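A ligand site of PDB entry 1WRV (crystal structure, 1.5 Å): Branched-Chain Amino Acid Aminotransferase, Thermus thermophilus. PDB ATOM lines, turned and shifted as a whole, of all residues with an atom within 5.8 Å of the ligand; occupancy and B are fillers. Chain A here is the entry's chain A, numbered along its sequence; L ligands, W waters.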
ATOM      1  N   PHE A  36      20.104  18.882 -21.319  1.00  0.00           N
ATOM      2  CA  PHE A  36      21.106  19.816 -20.868  1.00  0.00           C
ATOM      3  C   PHE A  36      22.419  19.130 -20.623  1.00  0.00           C
ATOM      4  O   PHE A  36      22.518  17.908 -20.698  1.00  0.00           O
ATOM      5  CB  PHE A  36      20.644  20.516 -19.588  1.00  0.00           C
ATOM      6  CG  PHE A  36      20.518  19.603 -18.397  1.00  0.00           C
ATOM      7  CD1 PHE A  36      21.601  19.372 -17.551  1.00  0.00           C
ATOM      8  CD2 PHE A  36      19.319  18.961 -18.117  1.00  0.00           C
ATOM      9  CE1 PHE A  36      21.495  18.529 -16.440  1.00  0.00           C
ATOM     10  CE2 PHE A  36      19.191  18.113 -17.011  1.00  0.00           C
ATOM     11  CZ  PHE A  36      20.290  17.900 -16.170  1.00  0.00           C
ATOM     12  N   GLU A  37      23.425  19.936 -20.328  1.00  0.00           N
ATOM     13  CA  GLU A  37      24.741  19.421 -20.005  1.00  0.00           C
ATOM     14  C   GLU A  37      25.310  20.247 -18.862  1.00  0.00           C
ATOM     15  O   GLU A  37      24.815  21.322 -18.541  1.00  0.00           O
ATOM     16  CB  GLU A  37      25.675  19.494 -21.223  1.00  0.00           C
ATOM     17  CG  GLU A  37      25.611  18.233 -22.065  1.00  0.00           C
ATOM     18  CD  GLU A  37      26.073  16.995 -21.307  1.00  0.00           C
ATOM     19  OE1 GLU A  37      25.664  15.886 -21.689  1.00  0.00           O
ATOM     20  OE2 GLU A  37      26.857  17.130 -20.344  1.00  0.00           O
ATOM     21  N   GLY A  38      26.340  19.681 -18.226  1.00  0.00           N
ATOM     22  CA  GLY A  38      27.022  20.337 -17.133  1.00  0.00           C
ATOM     23  C   GLY A  38      28.474  20.259 -17.543  1.00  0.00           C
ATOM     24  O   GLY A  38      29.046  19.170 -17.627  1.00  0.00           O
ATOM     25  N   HIS A  56      31.193  16.218 -23.878  1.00  0.00           N
ATOM     26  CA  HIS A  56      29.950  16.791 -23.377  1.00  0.00           C
ATOM     27  C   HIS A  56      29.011  17.215 -24.497  1.00  0.00           C
ATOM     28  O   HIS A  56      27.795  16.999 -24.410  1.00  0.00           O
ATOM     29  CB  HIS A  56      30.227  17.982 -22.454  1.00  0.00           C
ATOM     30  CG  HIS A  56      30.496  17.576 -21.034  1.00  0.00           C
ATOM     31  ND1 HIS A  56      31.762  17.471 -20.515  1.00  0.00           N
ATOM     32  CD2 HIS A  56      29.644  17.205 -20.045  1.00  0.00           C
ATOM     33  CE1 HIS A  56      31.688  17.042 -19.270  1.00  0.00           C
ATOM     34  NE2 HIS A  56      30.420  16.878 -18.956  1.00  0.00           N
ATOM     35  N   ARG A  59      27.369  14.202 -26.100  1.00  0.00           N
ATOM     36  CA  ARG A  59      26.283  13.694 -25.278  1.00  0.00           C
ATOM     37  C   ARG A  59      25.071  14.607 -25.343  1.00  0.00           C
ATOM     38  O   ARG A  59      23.936  14.154 -25.244  1.00  0.00           O
ATOM     39  CB  ARG A  59      26.759  13.526 -23.828  1.00  0.00           C
ATOM     40  CG  ARG A  59      25.809  12.692 -22.982  1.00  0.00           C
ATOM     41  CD  ARG A  59      26.455  12.313 -21.661  1.00  0.00           C
ATOM     42  NE  ARG A  59      26.712  13.473 -20.811  1.00  0.00           N
ATOM     43  CZ  ARG A  59      27.398  13.422 -19.674  1.00  0.00           C
ATOM     44  NH1 ARG A  59      27.918  12.273 -19.272  1.00  0.00           N
ATOM     45  NH2 ARG A  59      27.568  14.512 -18.941  1.00  0.00           N
ATOM     46  N   ARG A 148      15.831   4.671  -9.183  1.00  0.00           N
ATOM     47  CA  ARG A 148      16.139   5.284 -10.466  1.00  0.00           C
ATOM     48  C   ARG A 148      15.317   4.508 -11.499  1.00  0.00           C
ATOM     49  O   ARG A 148      15.176   3.296 -11.411  1.00  0.00           O
ATOM     50  CB  ARG A 148      17.630   5.203 -10.810  1.00  0.00           C
ATOM     51  CG  ARG A 148      17.944   5.964 -12.123  1.00  0.00           C
ATOM     52  CD  ARG A 148      19.428   6.243 -12.310  1.00  0.00           C
ATOM     53  NE  ARG A 148      19.738   6.793 -13.630  1.00  0.00           N
ATOM     54  CZ  ARG A 148      19.673   8.085 -13.965  1.00  0.00           C
ATOM     55  NH1 ARG A 148      19.299   8.995 -13.071  1.00  0.00           N
ATOM     56  NH2 ARG A 148      19.994   8.457 -15.192  1.00  0.00           N
ATOM     57  N   LYS A 159      20.651  13.212 -20.524  1.00  0.00           N
ATOM     58  CA  LYS A 159      20.363  14.249 -19.547  1.00  0.00           C
ATOM     59  C   LYS A 159      19.102  14.977 -20.003  1.00  0.00           C
ATOM     60  O   LYS A 159      19.159  16.111 -20.470  1.00  0.00           O
ATOM     61  CB  LYS A 159      21.525  15.242 -19.440  1.00  0.00           C
ATOM     62  CG  LYS A 159      22.658  14.797 -18.522  1.00  0.00           C
ATOM     63  CD  LYS A 159      23.545  15.993 -18.173  1.00  0.00           C
ATOM     64  CE  LYS A 159      24.786  15.637 -17.372  1.00  0.00           C
ATOM     65  NZ  LYS A 159      24.477  14.753 -16.252  1.00  0.00           N
ATOM     66  N   TYR A 164      14.984  14.440 -14.184  1.00  0.00           N
ATOM     67  CA  TYR A 164      15.376  14.976 -12.890  1.00  0.00           C
ATOM     68  C   TYR A 164      14.322  15.205 -11.821  1.00  0.00           C
ATOM     69  O   TYR A 164      14.619  15.683 -10.737  1.00  0.00           O
ATOM     70  CB  TYR A 164      16.271  16.199 -13.119  1.00  0.00           C
ATOM     71  CG  TYR A 164      17.495  15.730 -13.870  1.00  0.00           C
ATOM     72  CD1 TYR A 164      17.424  15.463 -15.240  1.00  0.00           C
ATOM     73  CD2 TYR A 164      18.648  15.349 -13.187  1.00  0.00           C
ATOM     74  CE1 TYR A 164      18.450  14.811 -15.900  1.00  0.00           C
ATOM     75  CE2 TYR A 164      19.685  14.688 -13.845  1.00  0.00           C
ATOM     76  CZ  TYR A 164      19.569  14.426 -15.203  1.00  0.00           C
ATOM     77  OH  TYR A 164      20.542  13.711 -15.856  1.00  0.00           O
ATOM     78  N   SER A 167      15.456  12.624  -9.619  1.00  0.00           N
ATOM     79  CA  SER A 167      16.630  13.085  -8.881  1.00  0.00           C
ATOM     80  C   SER A 167      16.242  14.114  -7.816  1.00  0.00           C
ATOM     81  O   SER A 167      16.770  14.080  -6.699  1.00  0.00           O
ATOM     82  CB  SER A 167      17.646  13.707  -9.848  1.00  0.00           C
ATOM     83  OG  SER A 167      18.263  12.710 -10.650  1.00  0.00           O
ATOM     84  N   GLU A 193      22.883   4.856  -8.637  1.00  0.00           N
ATOM     85  CA  GLU A 193      23.809   5.986  -8.546  1.00  0.00           C
ATOM     86  C   GLU A 193      23.215   7.060  -7.641  1.00  0.00           C
ATOM     87  O   GLU A 193      22.146   6.879  -7.074  1.00  0.00           O
ATOM     88  CB  GLU A 193      24.066   6.580  -9.931  1.00  0.00           C
ATOM     89  CG  GLU A 193      22.843   7.170 -10.607  1.00  0.00           C
ATOM     90  CD  GLU A 193      23.239   8.104 -11.730  1.00  0.00           C
ATOM     91  OE1 GLU A 193      23.926   9.101 -11.424  1.00  0.00           O
ATOM     92  OE2 GLU A 193      22.886   7.852 -12.895  1.00  0.00           O
ATOM     93  N   GLY A 194      23.922   8.185  -7.503  1.00  0.00           N
ATOM     94  CA  GLY A 194      23.417   9.277  -6.688  1.00  0.00           C
ATOM     95  C   GLY A 194      22.435  10.077  -7.517  1.00  0.00           C
ATOM     96  O   GLY A 194      22.181   9.736  -8.664  1.00  0.00           O
ATOM     97  N   SER A 195      21.859  11.142  -6.945  1.00  0.00           N
ATOM     98  CA  SER A 195      20.900  11.943  -7.703  1.00  0.00           C
ATOM     99  C   SER A 195      21.547  12.514  -8.962  1.00  0.00           C
ATOM    100  O   SER A 195      20.868  12.844  -9.926  1.00  0.00           O
ATOM    101  CB  SER A 195      20.339  13.080  -6.845  1.00  0.00           C
ATOM    102  OG  SER A 195      21.313  14.073  -6.597  1.00  0.00           O
ATOM    103  N   GLY A 196      22.870  12.625  -8.955  1.00  0.00           N
ATOM    104  CA  GLY A 196      23.565  13.153 -10.124  1.00  0.00           C
ATOM    105  C   GLY A 196      25.043  12.813 -10.100  1.00  0.00           C
ATOM    106  O   GLY A 196      25.869  13.576 -10.600  1.00  0.00           O
ATOM    107  N   GLU A 197      25.375  11.652  -9.524  1.00  0.00           N
ATOM    108  CA  GLU A 197      26.764  11.219  -9.442  1.00  0.00           C
ATOM    109  C   GLU A 197      26.877   9.710  -9.598  1.00  0.00           C
ATOM    110  O   GLU A 197      26.029   8.961  -9.120  1.00  0.00           O
ATOM    111  CB  GLU A 197      27.374  11.597  -8.088  1.00  0.00           C
ATOM    112  CG  GLU A 197      27.226  13.051  -7.676  1.00  0.00           C
ATOM    113  CD  GLU A 197      26.024  13.298  -6.796  1.00  0.00           C
ATOM    114  OE1 GLU A 197      25.977  14.346  -6.120  1.00  0.00           O
ATOM    115  OE2 GLU A 197      25.097  12.457  -6.771  1.00  0.00           O
ATOM    116  N   ASN A 198      27.937   9.264 -10.275  1.00  0.00           N
ATOM    117  CA  ASN A 198      28.177   7.836 -10.456  1.00  0.00           C
ATOM    118  C   ASN A 198      28.924   7.353  -9.221  1.00  0.00           C
ATOM    119  O   ASN A 198      29.634   8.128  -8.582  1.00  0.00           O
ATOM    120  CB  ASN A 198      29.011   7.594 -11.716  1.00  0.00           C
ATOM    121  CG  ASN A 198      28.264   7.955 -12.982  1.00  0.00           C
ATOM    122  OD1 ASN A 198      28.769   8.688 -13.823  1.00  0.00           O
ATOM    123  ND2 ASN A 198      27.048   7.440 -13.128  1.00  0.00           N
ATOM    124  N   LEU A 216      23.639   7.236 -15.800  1.00  0.00           N
ATOM    125  CA  LEU A 216      24.170   8.023 -16.902  1.00  0.00           C
ATOM    126  C   LEU A 216      25.633   7.619 -17.009  1.00  0.00           C
ATOM    127  O   LEU A 216      26.270   7.338 -16.004  1.00  0.00           O
ATOM    128  CB  LEU A 216      24.087   9.517 -16.598  1.00  0.00           C
ATOM    129  CG  LEU A 216      24.319  10.390 -17.833  1.00  0.00           C
ATOM    130  CD1 LEU A 216      22.990  10.595 -18.542  1.00  0.00           C
ATOM    131  CD2 LEU A 216      24.898  11.732 -17.437  1.00  0.00           C
ATOM    132  N   GLU A 217      26.154   7.582 -18.232  1.00  0.00           N
ATOM    133  CA  GLU A 217      27.558   7.225 -18.447  1.00  0.00           C
ATOM    134  C   GLU A 217      28.390   8.468 -18.177  1.00  0.00           C
ATOM    135  O   GLU A 217      28.660   9.253 -19.070  1.00  0.00           O
ATOM    136  CB  GLU A 217      27.778   6.761 -19.892  1.00  0.00           C
ATOM    137  CG  GLU A 217      27.001   5.521 -20.272  1.00  0.00           C
ATOM    138  CD  GLU A 217      27.285   5.054 -21.687  1.00  0.00           C
ATOM    139  OE1 GLU A 217      26.825   3.963 -22.066  1.00  0.00           O
ATOM    140  OE2 GLU A 217      27.979   5.794 -22.430  1.00  0.00           O
ATOM    141  N   GLY A 218      28.799   8.628 -16.933  1.00  0.00           N
ATOM    142  CA  GLY A 218      29.558   9.810 -16.560  1.00  0.00           C
ATOM    143  C   GLY A 218      30.903  10.032 -17.221  1.00  0.00           C
ATOM    144  O   GLY A 218      31.677   9.099 -17.438  1.00  0.00           O
ATOM    145  N   ILE A 219      31.167  11.285 -17.551  1.00  0.00           N
ATOM    146  CA  ILE A 219      32.437  11.655 -18.163  1.00  0.00           C
ATOM    147  C   ILE A 219      33.478  11.723 -17.059  1.00  0.00           C
ATOM    148  O   ILE A 219      34.657  11.454 -17.272  1.00  0.00           O
ATOM    149  CB  ILE A 219      32.295  12.989 -18.923  1.00  0.00           C
ATOM    150  CG1 ILE A 219      31.512  12.746 -20.210  1.00  0.00           C
ATOM    151  CG2 ILE A 219      33.669  13.584 -19.204  1.00  0.00           C
ATOM    152  CD1 ILE A 219      30.979  14.003 -20.869  1.00  0.00           C
ATOM    153  N   THR A 220      33.046  12.069 -15.848  1.00  0.00           N
ATOM    154  CA  THR A 220      33.956  12.132 -14.716  1.00  0.00           C
ATOM    155  C   THR A 220      34.295  10.686 -14.347  1.00  0.00           C
ATOM    156  O   THR A 220      35.435  10.371 -14.043  1.00  0.00           O
ATOM    157  CB  THR A 220      33.303  12.839 -13.513  1.00  0.00           C
ATOM    158  OG1 THR A 220      32.721  14.073 -13.950  1.00  0.00           O
ATOM    159  CG2 THR A 220      34.344  13.157 -12.450  1.00  0.00           C
ATOM    160  N   ARG A 221      33.294   9.816 -14.390  1.00  0.00           N
ATOM    161  CA  ARG A 221      33.499   8.399 -14.112  1.00  0.00           C
ATOM    162  C   ARG A 221      34.544   7.854 -15.091  1.00  0.00           C
ATOM    163  O   ARG A 221      35.503   7.195 -14.698  1.00  0.00           O
ATOM    164  CB  ARG A 221      32.177   7.633 -14.293  1.00  0.00           C
ATOM    165  CG  ARG A 221      32.293   6.104 -14.282  1.00  0.00           C
ATOM    166  CD  ARG A 221      30.943   5.461 -14.546  1.00  0.00           C
ATOM    167  NE  ARG A 221      30.985   3.995 -14.467  1.00  0.00           N
ATOM    168  CZ  ARG A 221      31.499   3.211 -15.405  1.00  0.00           C
ATOM    169  NH1 ARG A 221      32.021   3.716 -16.505  1.00  0.00           N
ATOM    170  NH2 ARG A 221      31.510   1.894 -15.218  1.00  0.00           N
ATOM    171  N   THR A 254      31.381  10.453  -8.448  1.00  0.00           N
ATOM    172  CA  THR A 254      31.984  11.304  -9.461  1.00  0.00           C
ATOM    173  C   THR A 254      30.886  11.997 -10.246  1.00  0.00           C
ATOM    174  O   THR A 254      29.800  11.455 -10.453  1.00  0.00           O
ATOM    175  CB  THR A 254      32.845  10.499 -10.453  1.00  0.00           C
ATOM    176  OG1 THR A 254      32.036   9.535 -11.139  1.00  0.00           O
ATOM    177  CG2 THR A 254      33.974   9.788  -9.712  1.00  0.00           C
ATOM    178  N   GLY A 255      31.189  13.213 -10.680  1.00  0.00           N
ATOM    179  CA  GLY A 255      30.253  14.006 -11.453  1.00  0.00           C
ATOM    180  C   GLY A 255      30.961  15.297 -11.801  1.00  0.00           C
ATOM    181  O   GLY A 255      31.957  15.653 -11.156  1.00  0.00           O
ATOM    182  N   THR A 256      30.482  16.017 -12.814  1.00  0.00           N
ATOM    183  CA  THR A 256      31.152  17.259 -13.177  1.00  0.00           C
ATOM    184  C   THR A 256      31.146  18.256 -12.025  1.00  0.00           C
ATOM    185  O   THR A 256      32.165  18.901 -11.762  1.00  0.00           O
ATOM    186  CB  THR A 256      30.501  17.876 -14.427  1.00  0.00           C
ATOM    187  OG1 THR A 256      30.756  17.020 -15.551  1.00  0.00           O
ATOM    188  CG2 THR A 256      31.078  19.262 -14.716  1.00  0.00           C
ATOM    189  N   ALA A 257      30.027  18.376 -11.326  1.00  0.00           N
ATOM    190  CA  ALA A 257      29.949  19.292 -10.192  1.00  0.00           C
ATOM    191  C   ALA A 257      30.640  18.706  -8.963  1.00  0.00           C
ATOM    192  O   ALA A 257      31.331  19.415  -8.227  1.00  0.00           O
ATOM    193  CB  ALA A 257      28.491  19.601  -9.866  1.00  0.00           C
HETATM  194  N1  LIG L   1      24.397  10.959 -13.032  1.00  0.00           N
HETATM  195  C1  LIG L   1      23.395  11.737 -13.507  1.00  0.00           C
HETATM  196  C2  LIG L   1      21.958  11.311 -13.279  1.00  0.00           C
HETATM  197  C3  LIG L   1      23.686  12.910 -14.180  1.00  0.00           C
HETATM  198  O1  LIG L   1      22.681  13.697 -14.651  1.00  0.00           O
HETATM  199  C4  LIG L   1      25.017  13.281 -14.379  1.00  0.00           C
HETATM  200  C5  LIG L   1      25.321  14.573 -15.177  1.00  0.00           C
HETATM  201  C6  LIG L   1      26.030  12.454 -13.885  1.00  0.00           C
HETATM  202  C7  LIG L   1      25.698  11.308 -13.225  1.00  0.00           C
HETATM  203  C8  LIG L   1      27.528  12.734 -14.007  1.00  0.00           C
HETATM  204  O2  LIG L   1      28.031  12.762 -15.326  1.00  0.00           O
HETATM  205  P1  LIG L   1      29.347  13.638 -15.602  1.00  0.00           P
HETATM  206  O3  LIG L   1      29.076  15.047 -15.222  1.00  0.00           O
HETATM  207  O4  LIG L   1      29.462  13.446 -17.163  1.00  0.00           O
HETATM  208  O5  LIG L   1      30.468  12.940 -14.900  1.00  0.00           O
HETATM  209  O   HOH W   1      27.674  16.865 -16.897  1.00  0.00           O
HETATM  210  O   HOH W   2      30.614  10.628 -13.454  1.00  0.00           O
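NE2 of His 56 touches O4 of the ligand (3.99 Å).
Arg 148 touches the ligand.
Ser 195 touches the ligand (O to C2, 3.8 Å).
Gly 196 touches the ligand.
Glu 197 touches the ligand.
Leu 216 touches the ligand.
Gly 218 touches the ligand (CA to O2, 3.5 Å).
Gly 255 touches the ligand (CA to O5, 3.6 Å).
Hydrophobic or aromatic side chains that line the ligand: Tyr 164, Leu 216 and Ile 219.
15 residues have an atom within 4 Å of the ligand: His 56, Arg 59, Arg 148, Lys 159, Tyr 164, Glu 193, Ser 195, Gly 196, Glu 197, Leu 216, Gly 218, Ile 219, Thr 220, Gly 255 and Thr 256.
Water W2 lies within hydrogen-bond range of OD1 of Asn 198 (2.7 Å), O5 of the ligand (2.7 Å), OG1 of Thr 254 (2.9 Å) and N of Arg 221 (3.0 Å).
Water W1 lies within hydrogen-bond range of the backbone carbonyl oxygen of Gly 38 (2.8 Å), an oxygen (O3) of the ligand (2.8 Å), the guanidinium group of Arg 59 (3.1 Å), the side-chain hydroxyl of Thr 256 (3.4 Å) and a ring nitrogen (NE2) of His 56 (3.4 Å).
The guanidinium group of Arg 59 lies within hydrogen-bond range of the backbone carbonyl oxygen of Glu 217 (3.1 Å).
The backbone carbonyl oxygen (O) of Lys 159 sits at hydrogen-bond distance from the backbone NH (N) of Phe 36.
The side-chain carboxylate of Glu 193 is in salt-bridge range of the guanidinium group of Arg 148, at 3.4 Å.
The backbone carbonyl oxygen (O) of Leu 216 is in hydrogen-bond range of the side-chain amide nitrogen (ND2) of Asn 198.
N of Leu 216 lies within hydrogen-bond range of OE2 of Glu 193, 3.1 Å away.
The side-chain carboxylate of Glu 193 lies within hydrogen-bond range of the backbone NH of Glu 197.
OE1 of Glu 37 lies within salt-bridge range of NE of Arg 59, at 2.8 Å.
OG1 of Thr 220 is in hydrogen-bond range of N of Thr 256 (3.2 Å).
N of Thr 220 lies within hydrogen-bond range of O5 of the ligand.
The side-chain amino group (NZ) of Lys 159 is bonded to a carbon (C5) of the ligand, 1.4 Å away.
The side-chain carboxylate of Glu 193 sits at hydrogen-bond distance from a nitrogen (N1) of the ligand (2.5 Å).
The side-chain hydroxyl (OH) of Tyr 164 lies within hydrogen-bond range of an oxygen (O1) of the ligand, at 2.5 Å.
An oxygen (O5) of the ligand lies within hydrogen-bond range of the side-chain hydroxyl (OG1) of Thr 220 (2.7 Å).
An oxygen (O4) of the ligand lies within hydrogen-bond range of the backbone NH (N) of Ile 219, at 2.8 Å.
An oxygen (O4) of the ligand lies within salt-bridge range of the guanidinium group (NH2) of Arg 59, 2.8 Å away.
N of Thr 256 sits at hydrogen-bond distance from O3 of the ligand (3.0 Å).
OG1 of Thr 256 is in hydrogen-bond range of O3 of the ligand, 2.6 Å away.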
